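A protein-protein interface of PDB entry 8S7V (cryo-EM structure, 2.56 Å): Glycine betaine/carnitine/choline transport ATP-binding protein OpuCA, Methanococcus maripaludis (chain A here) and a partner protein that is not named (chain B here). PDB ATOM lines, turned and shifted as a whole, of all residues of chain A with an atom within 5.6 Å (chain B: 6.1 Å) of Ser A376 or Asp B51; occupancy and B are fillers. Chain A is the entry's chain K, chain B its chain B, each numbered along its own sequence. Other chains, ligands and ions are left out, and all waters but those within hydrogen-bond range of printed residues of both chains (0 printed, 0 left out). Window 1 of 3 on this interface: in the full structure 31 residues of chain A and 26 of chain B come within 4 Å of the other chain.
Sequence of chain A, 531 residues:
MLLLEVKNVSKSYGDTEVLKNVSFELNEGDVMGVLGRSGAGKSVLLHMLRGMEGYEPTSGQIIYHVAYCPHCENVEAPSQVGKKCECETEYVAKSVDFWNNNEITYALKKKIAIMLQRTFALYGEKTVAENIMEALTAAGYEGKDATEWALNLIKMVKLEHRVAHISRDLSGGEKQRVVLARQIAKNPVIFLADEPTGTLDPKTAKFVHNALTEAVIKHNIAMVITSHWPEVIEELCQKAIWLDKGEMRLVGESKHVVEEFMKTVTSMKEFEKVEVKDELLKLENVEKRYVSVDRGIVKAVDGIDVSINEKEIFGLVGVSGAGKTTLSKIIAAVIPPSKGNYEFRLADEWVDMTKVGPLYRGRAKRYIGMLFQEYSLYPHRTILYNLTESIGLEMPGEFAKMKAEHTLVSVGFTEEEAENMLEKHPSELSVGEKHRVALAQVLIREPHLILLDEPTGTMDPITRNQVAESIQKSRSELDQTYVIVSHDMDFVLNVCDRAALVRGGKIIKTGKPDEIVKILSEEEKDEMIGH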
ATOM      1  N   ARG A 118      -4.513 -15.288  13.198  1.00  0.00           N
ATOM      2  CA  ARG A 118      -5.417 -14.162  13.461  1.00  0.00           C
ATOM      3  C   ARG A 118      -4.670 -12.930  13.979  1.00  0.00           C
ATOM      4  O   ARG A 118      -5.268 -11.887  14.254  1.00  0.00           O
ATOM      5  CB  ARG A 118      -6.550 -14.578  14.410  1.00  0.00           C
ATOM      6  CG  ARG A 118      -6.423 -14.140  15.866  1.00  0.00           C
ATOM      7  CD  ARG A 118      -7.768 -14.232  16.570  1.00  0.00           C
ATOM      8  NE  ARG A 118      -7.749 -13.618  17.892  1.00  0.00           N
ATOM      9  CZ  ARG A 118      -8.061 -12.353  18.134  1.00  0.00           C
ATOM     10  NH1 ARG A 118      -8.414 -11.529  17.161  1.00  0.00           N
ATOM     11  NH2 ARG A 118      -8.020 -11.903  19.384  1.00  0.00           N
ATOM     12  N   GLU A 374     -12.105  -8.636  13.328  1.00  0.00           N
ATOM     13  CA  GLU A 374     -10.957  -8.647  14.229  1.00  0.00           C
ATOM     14  C   GLU A 374     -11.483  -8.423  15.643  1.00  0.00           C
ATOM     15  O   GLU A 374     -11.392  -7.336  16.211  1.00  0.00           O
ATOM     16  CB  GLU A 374      -9.935  -7.592  13.822  1.00  0.00           C
ATOM     17  CG  GLU A 374      -8.992  -8.030  12.714  1.00  0.00           C
ATOM     18  CD  GLU A 374      -9.575  -7.809  11.331  1.00  0.00           C
ATOM     19  OE1 GLU A 374      -9.547  -8.753  10.514  1.00  0.00           O
ATOM     20  OE2 GLU A 374     -10.058  -6.689  11.061  1.00  0.00           O
ATOM     21  N   TYR A 375     -12.059  -9.478  16.207  1.00  0.00           N
ATOM     22  CA  TYR A 375     -12.639  -9.412  17.538  1.00  0.00           C
ATOM     23  C   TYR A 375     -11.540  -9.390  18.597  1.00  0.00           C
ATOM     24  O   TYR A 375     -10.368  -9.661  18.327  1.00  0.00           O
ATOM     25  CB  TYR A 375     -13.570 -10.598  17.772  1.00  0.00           C
ATOM     26  CG  TYR A 375     -12.870 -11.934  17.690  1.00  0.00           C
ATOM     27  CD1 TYR A 375     -12.673 -12.561  16.469  1.00  0.00           C
ATOM     28  CD2 TYR A 375     -12.399 -12.564  18.833  1.00  0.00           C
ATOM     29  CE1 TYR A 375     -12.028 -13.778  16.389  1.00  0.00           C
ATOM     30  CE2 TYR A 375     -11.755 -13.780  18.762  1.00  0.00           C
ATOM     31  CZ  TYR A 375     -11.572 -14.383  17.537  1.00  0.00           C
ATOM     32  OH  TYR A 375     -10.931 -15.596  17.461  1.00  0.00           O
ATOM     33  N   SER A 376     -11.936  -9.061  19.824  1.00  0.00           N
ATOM     34  CA  SER A 376     -11.014  -9.119  20.948  1.00  0.00           C
ATOM     35  C   SER A 376     -11.807  -9.309  22.228  1.00  0.00           C
ATOM     36  O   SER A 376     -12.961  -8.888  22.339  1.00  0.00           O
ATOM     37  CB  SER A 376     -10.152  -7.860  21.045  1.00  0.00           C
ATOM     38  OG  SER A 376     -10.957  -6.702  21.168  1.00  0.00           O
ATOM     39  N   LEU A 377     -11.163  -9.949  23.194  1.00  0.00           N
ATOM     40  CA  LEU A 377     -11.682 -10.090  24.544  1.00  0.00           C
ATOM     41  C   LEU A 377     -10.792  -9.280  25.484  1.00  0.00           C
ATOM     42  O   LEU A 377      -9.865  -8.590  25.053  1.00  0.00           O
ATOM     43  CB  LEU A 377     -11.746 -11.564  24.947  1.00  0.00           C
ATOM     44  CG  LEU A 377     -12.507 -12.492  24.003  1.00  0.00           C
ATOM     45  CD1 LEU A 377     -12.252 -13.943  24.368  1.00  0.00           C
ATOM     46  CD2 LEU A 377     -13.993 -12.184  24.029  1.00  0.00           C
ATOM     47  N   TYR A 378     -11.081  -9.363  26.777  1.00  0.00           N
ATOM     48  CA  TYR A 378     -10.241  -8.719  27.772  1.00  0.00           C
ATOM     49  C   TYR A 378      -9.284  -9.757  28.332  1.00  0.00           C
ATOM     50  O   TYR A 378      -9.682 -10.542  29.206  1.00  0.00           O
ATOM     51  CB  TYR A 378     -11.090  -8.105  28.883  1.00  0.00           C
ATOM     52  CG  TYR A 378     -12.071  -7.072  28.373  1.00  0.00           C
ATOM     53  CD1 TYR A 378     -11.705  -5.738  28.250  1.00  0.00           C
ATOM     54  CD2 TYR A 378     -13.356  -7.434  27.998  1.00  0.00           C
ATOM     55  CE1 TYR A 378     -12.596  -4.793  27.777  1.00  0.00           C
ATOM     56  CE2 TYR A 378     -14.254  -6.497  27.524  1.00  0.00           C
ATOM     57  CZ  TYR A 378     -13.869  -5.180  27.414  1.00  0.00           C
ATOM     58  OH  TYR A 378     -14.763  -4.246  26.943  1.00  0.00           O
ATOM     59  N   ALA A 438     -16.414 -15.049  22.002  1.00  0.00           N
ATOM     60  CA  ALA A 438     -16.845 -13.724  21.562  1.00  0.00           C
ATOM     61  C   ALA A 438     -18.268 -13.757  21.018  1.00  0.00           C
ATOM     62  O   ALA A 438     -19.053 -12.826  21.248  1.00  0.00           O
ATOM     63  CB  ALA A 438     -15.878 -13.181  20.511  1.00  0.00           C
ATOM     64  N   GLN A 441     -20.434 -13.771  23.930  1.00  0.00           N
ATOM     65  CA  GLN A 441     -20.471 -12.435  24.513  1.00  0.00           C
ATOM     66  C   GLN A 441     -21.452 -11.541  23.768  1.00  0.00           C
ATOM     67  O   GLN A 441     -22.171 -10.746  24.384  1.00  0.00           O
ATOM     68  CB  GLN A 441     -19.073 -11.821  24.503  1.00  0.00           C
ATOM     69  CG  GLN A 441     -18.949 -10.535  25.293  1.00  0.00           C
ATOM     70  CD  GLN A 441     -17.511 -10.092  25.458  1.00  0.00           C
ATOM     71  OE1 GLN A 441     -16.614 -10.915  25.631  1.00  0.00           O
ATOM     72  NE2 GLN A 441     -17.284  -8.787  25.404  1.00  0.00           N
ATOM     73  N   ARG B  46     -11.061   3.538  21.346  1.00  0.00           N
ATOM     74  CA  ARG B  46     -11.391   2.408  20.491  1.00  0.00           C
ATOM     75  C   ARG B  46     -12.846   2.022  20.692  1.00  0.00           C
ATOM     76  O   ARG B  46     -13.449   2.300  21.732  1.00  0.00           O
ATOM     77  CB  ARG B  46     -10.490   1.200  20.774  1.00  0.00           C
ATOM     78  CG  ARG B  46     -10.585   0.681  22.193  1.00  0.00           C
ATOM     79  CD  ARG B  46      -9.842  -0.630  22.352  1.00  0.00           C
ATOM     80  NE  ARG B  46     -10.665  -1.775  21.983  1.00  0.00           N
ATOM     81  CZ  ARG B  46     -11.173  -2.642  22.848  1.00  0.00           C
ATOM     82  NH1 ARG B  46     -10.983  -2.510  24.150  1.00  0.00           N
ATOM     83  NH2 ARG B  46     -11.893  -3.663  22.395  1.00  0.00           N
ATOM     84  N   GLN B  47     -13.405   1.382  19.676  1.00  0.00           N
ATOM     85  CA  GLN B  47     -14.752   0.843  19.783  1.00  0.00           C
ATOM     86  C   GLN B  47     -14.710  -0.476  20.544  1.00  0.00           C
ATOM     87  O   GLN B  47     -13.950  -1.374  20.169  1.00  0.00           O
ATOM     88  CB  GLN B  47     -15.357   0.637  18.397  1.00  0.00           C
ATOM     89  CG  GLN B  47     -16.521  -0.332  18.368  1.00  0.00           C
ATOM     90  CD  GLN B  47     -17.842   0.337  18.681  1.00  0.00           C
ATOM     91  OE1 GLN B  47     -17.934   1.563  18.721  1.00  0.00           O
ATOM     92  NE2 GLN B  47     -18.873  -0.468  18.909  1.00  0.00           N
ATOM     93  N   GLY B  49     -15.247  -4.192  21.667  1.00  0.00           N
ATOM     94  CA  GLY B  49     -15.525  -5.386  20.908  1.00  0.00           C
ATOM     95  C   GLY B  49     -14.591  -5.630  19.742  1.00  0.00           C
ATOM     96  O   GLY B  49     -14.511  -6.764  19.258  1.00  0.00           O
ATOM     97  N   GLU B  50     -13.883  -4.605  19.281  1.00  0.00           N
ATOM     98  CA  GLU B  50     -12.925  -4.741  18.194  1.00  0.00           C
ATOM     99  C   GLU B  50     -11.510  -4.839  18.749  1.00  0.00           C
ATOM    100  O   GLU B  50     -11.231  -4.437  19.881  1.00  0.00           O
ATOM    101  CB  GLU B  50     -13.039  -3.565  17.220  1.00  0.00           C
ATOM    102  CG  GLU B  50     -12.243  -2.340  17.619  1.00  0.00           C
ATOM    103  CD  GLU B  50     -12.373  -1.214  16.614  1.00  0.00           C
ATOM    104  OE1 GLU B  50     -13.129  -1.376  15.632  1.00  0.00           O
ATOM    105  OE2 GLU B  50     -11.723  -0.165  16.807  1.00  0.00           O
ATOM    106  N   ASP B  51     -10.613  -5.388  17.935  1.00  0.00           N
ATOM    107  CA  ASP B  51      -9.270  -5.682  18.405  1.00  0.00           C
ATOM    108  C   ASP B  51      -8.445  -4.407  18.541  1.00  0.00           C
ATOM    109  O   ASP B  51      -8.719  -3.379  17.915  1.00  0.00           O
ATOM    110  CB  ASP B  51      -8.568  -6.660  17.464  1.00  0.00           C
ATOM    111  CG  ASP B  51      -7.413  -7.383  18.133  1.00  0.00           C
ATOM    112  OD1 ASP B  51      -7.050  -7.006  19.267  1.00  0.00           O
ATOM    113  OD2 ASP B  51      -6.869  -8.331  17.528  1.00  0.00           O
ATOM    114  N   TYR B  52      -7.416  -4.490  19.380  1.00  0.00           N
ATOM    115  CA  TYR B  52      -6.533  -3.356  19.607  1.00  0.00           C
ATOM    116  C   TYR B  52      -5.652  -3.118  18.389  1.00  0.00           C
ATOM    117  O   TYR B  52      -5.103  -4.059  17.812  1.00  0.00           O
ATOM    118  CB  TYR B  52      -5.666  -3.602  20.840  1.00  0.00           C
ATOM    119  CG  TYR B  52      -6.447  -3.773  22.119  1.00  0.00           C
ATOM    120  CD1 TYR B  52      -6.825  -2.674  22.875  1.00  0.00           C
ATOM    121  CD2 TYR B  52      -6.805  -5.032  22.573  1.00  0.00           C
ATOM    122  CE1 TYR B  52      -7.537  -2.826  24.046  1.00  0.00           C
ATOM    123  CE2 TYR B  52      -7.518  -5.194  23.743  1.00  0.00           C
ATOM    124  CZ  TYR B  52      -7.881  -4.086  24.474  1.00  0.00           C
ATOM    125  OH  TYR B  52      -8.591  -4.241  25.642  1.00  0.00           O
ATOM    126  N   LYS B  53      -5.523  -1.855  17.995  1.00  0.00           N
ATOM    127  CA  LYS B  53      -4.594  -1.504  16.934  1.00  0.00           C
ATOM    128  C   LYS B  53      -3.160  -1.641  17.427  1.00  0.00           C
ATOM    129  O   LYS B  53      -2.862  -1.449  18.608  1.00  0.00           O
ATOM    130  CB  LYS B  53      -4.850  -0.080  16.445  1.00  0.00           C
ATOM    131  CG  LYS B  53      -6.284   0.173  16.037  1.00  0.00           C
ATOM    132  CD  LYS B  53      -6.502   1.626  15.673  1.00  0.00           C
ATOM    133  CE  LYS B  53      -7.279   1.749  14.376  1.00  0.00           C
ATOM    134  NZ  LYS B  53      -8.198   0.595  14.183  1.00  0.00           N
ATOM    135  N   HIS B  83       0.681  -2.926  21.288  1.00  0.00           N
ATOM    136  CA  HIS B  83      -0.473  -1.989  21.203  1.00  0.00           C
ATOM    137  C   HIS B  83      -0.044  -0.520  21.250  1.00  0.00           C
ATOM    138  O   HIS B  83       0.999  -0.216  21.856  1.00  0.00           O
ATOM    139  CB  HIS B  83      -1.455  -2.275  22.341  1.00  0.00           C
ATOM    140  CG  HIS B  83      -2.023  -3.653  22.317  1.00  0.00           C
ATOM    141  ND1 HIS B  83      -2.527  -4.267  23.443  1.00  0.00           N
ATOM    142  CD2 HIS B  83      -2.174  -4.529  21.318  1.00  0.00           C
ATOM    143  CE1 HIS B  83      -2.961  -5.475  23.122  1.00  0.00           C
ATOM    144  NE2 HIS B  83      -2.758  -5.654  21.836  1.00  0.00           N
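The guanidinium group (NH2) of Arg B46 is in hydrogen-bond range of the backbone carbonyl oxygen (O) of Glu B50, 2.7 Å away.
The side-chain hydroxyl (OH) of Tyr B52 lies within hydrogen-bond range of the guanidinium group (NH1) of Arg B46, at 3.3 Å.
The backbone carbonyl oxygen of Tyr A375 lies within hydrogen-bond range of the guanidinium group of Arg A118 (2.9 Å).
Of chain B, only Arg B46 (3.4 Å), Gly B49 (3.5 Å), Glu B50 (2.6 Å) and Asp B51 (3.4 Å) come within 4 Å of Ser A376.
Of the printed residues of chain B, Tyr A375 touches Gly B49 and Asp B51.
Of the printed residues of chain B, Glu A374 touches Glu B50 (3.6 Å) and Asp B51 (2.7 Å).
Of the printed residues of chain A, Glu B50 touches Glu A374 (3.6 Å) and Ser A376 (2.6 Å).
Printed residues of chain A within 4 Å of Gly B49: Tyr A375 and Ser A376.
Tyr B52 touches none of the printed residues of chain A.
The nearest residue of chain B that does not touch Ser A376 is Tyr B52 (4.5 Å).
The nearest printed residue of chain A that does not touch Asp B51 is Leu A377 (6.4 Å).
The nearest printed residue of chain B that does not touch Glu A374 is Gly B49 (4.4 Å).
Among the printed residues, merely in contact across the chains: Glu A374 with Glu B50 (3.6 Å), Tyr A375 with Gly B49 (3.7 Å), Tyr A375 with Asp B51 (3.6 Å) and Ser A376 with Asp B51 (3.4 Å).
The guanidinium group (NH2) of Arg B46 lies within hydrogen-bond range of the side-chain hydroxyl (OG) of Ser A376 (3.4 Å).
The backbone carbonyl oxygen (O) of Gly B49 sits at hydrogen-bond distance from the backbone NH (N) of Ser A376 (3.5 Å).
O of Glu B50 sits at hydrogen-bond distance from OG of Ser A376 (2.6 Å).
The side-chain carboxylate of Asp B51 lies within salt-bridge range of the guanidinium group of Arg A118 (3.6 Å).
The backbone carbonyl oxygen of Glu A374 sits at hydrogen-bond distance from the backbone NH of Asp B51 (2.7 Å).
Of the 8 printed residues of chain A, 4 touch a printed residue of chain B.
Among the printed residues, 9 pairs touch across the chains.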
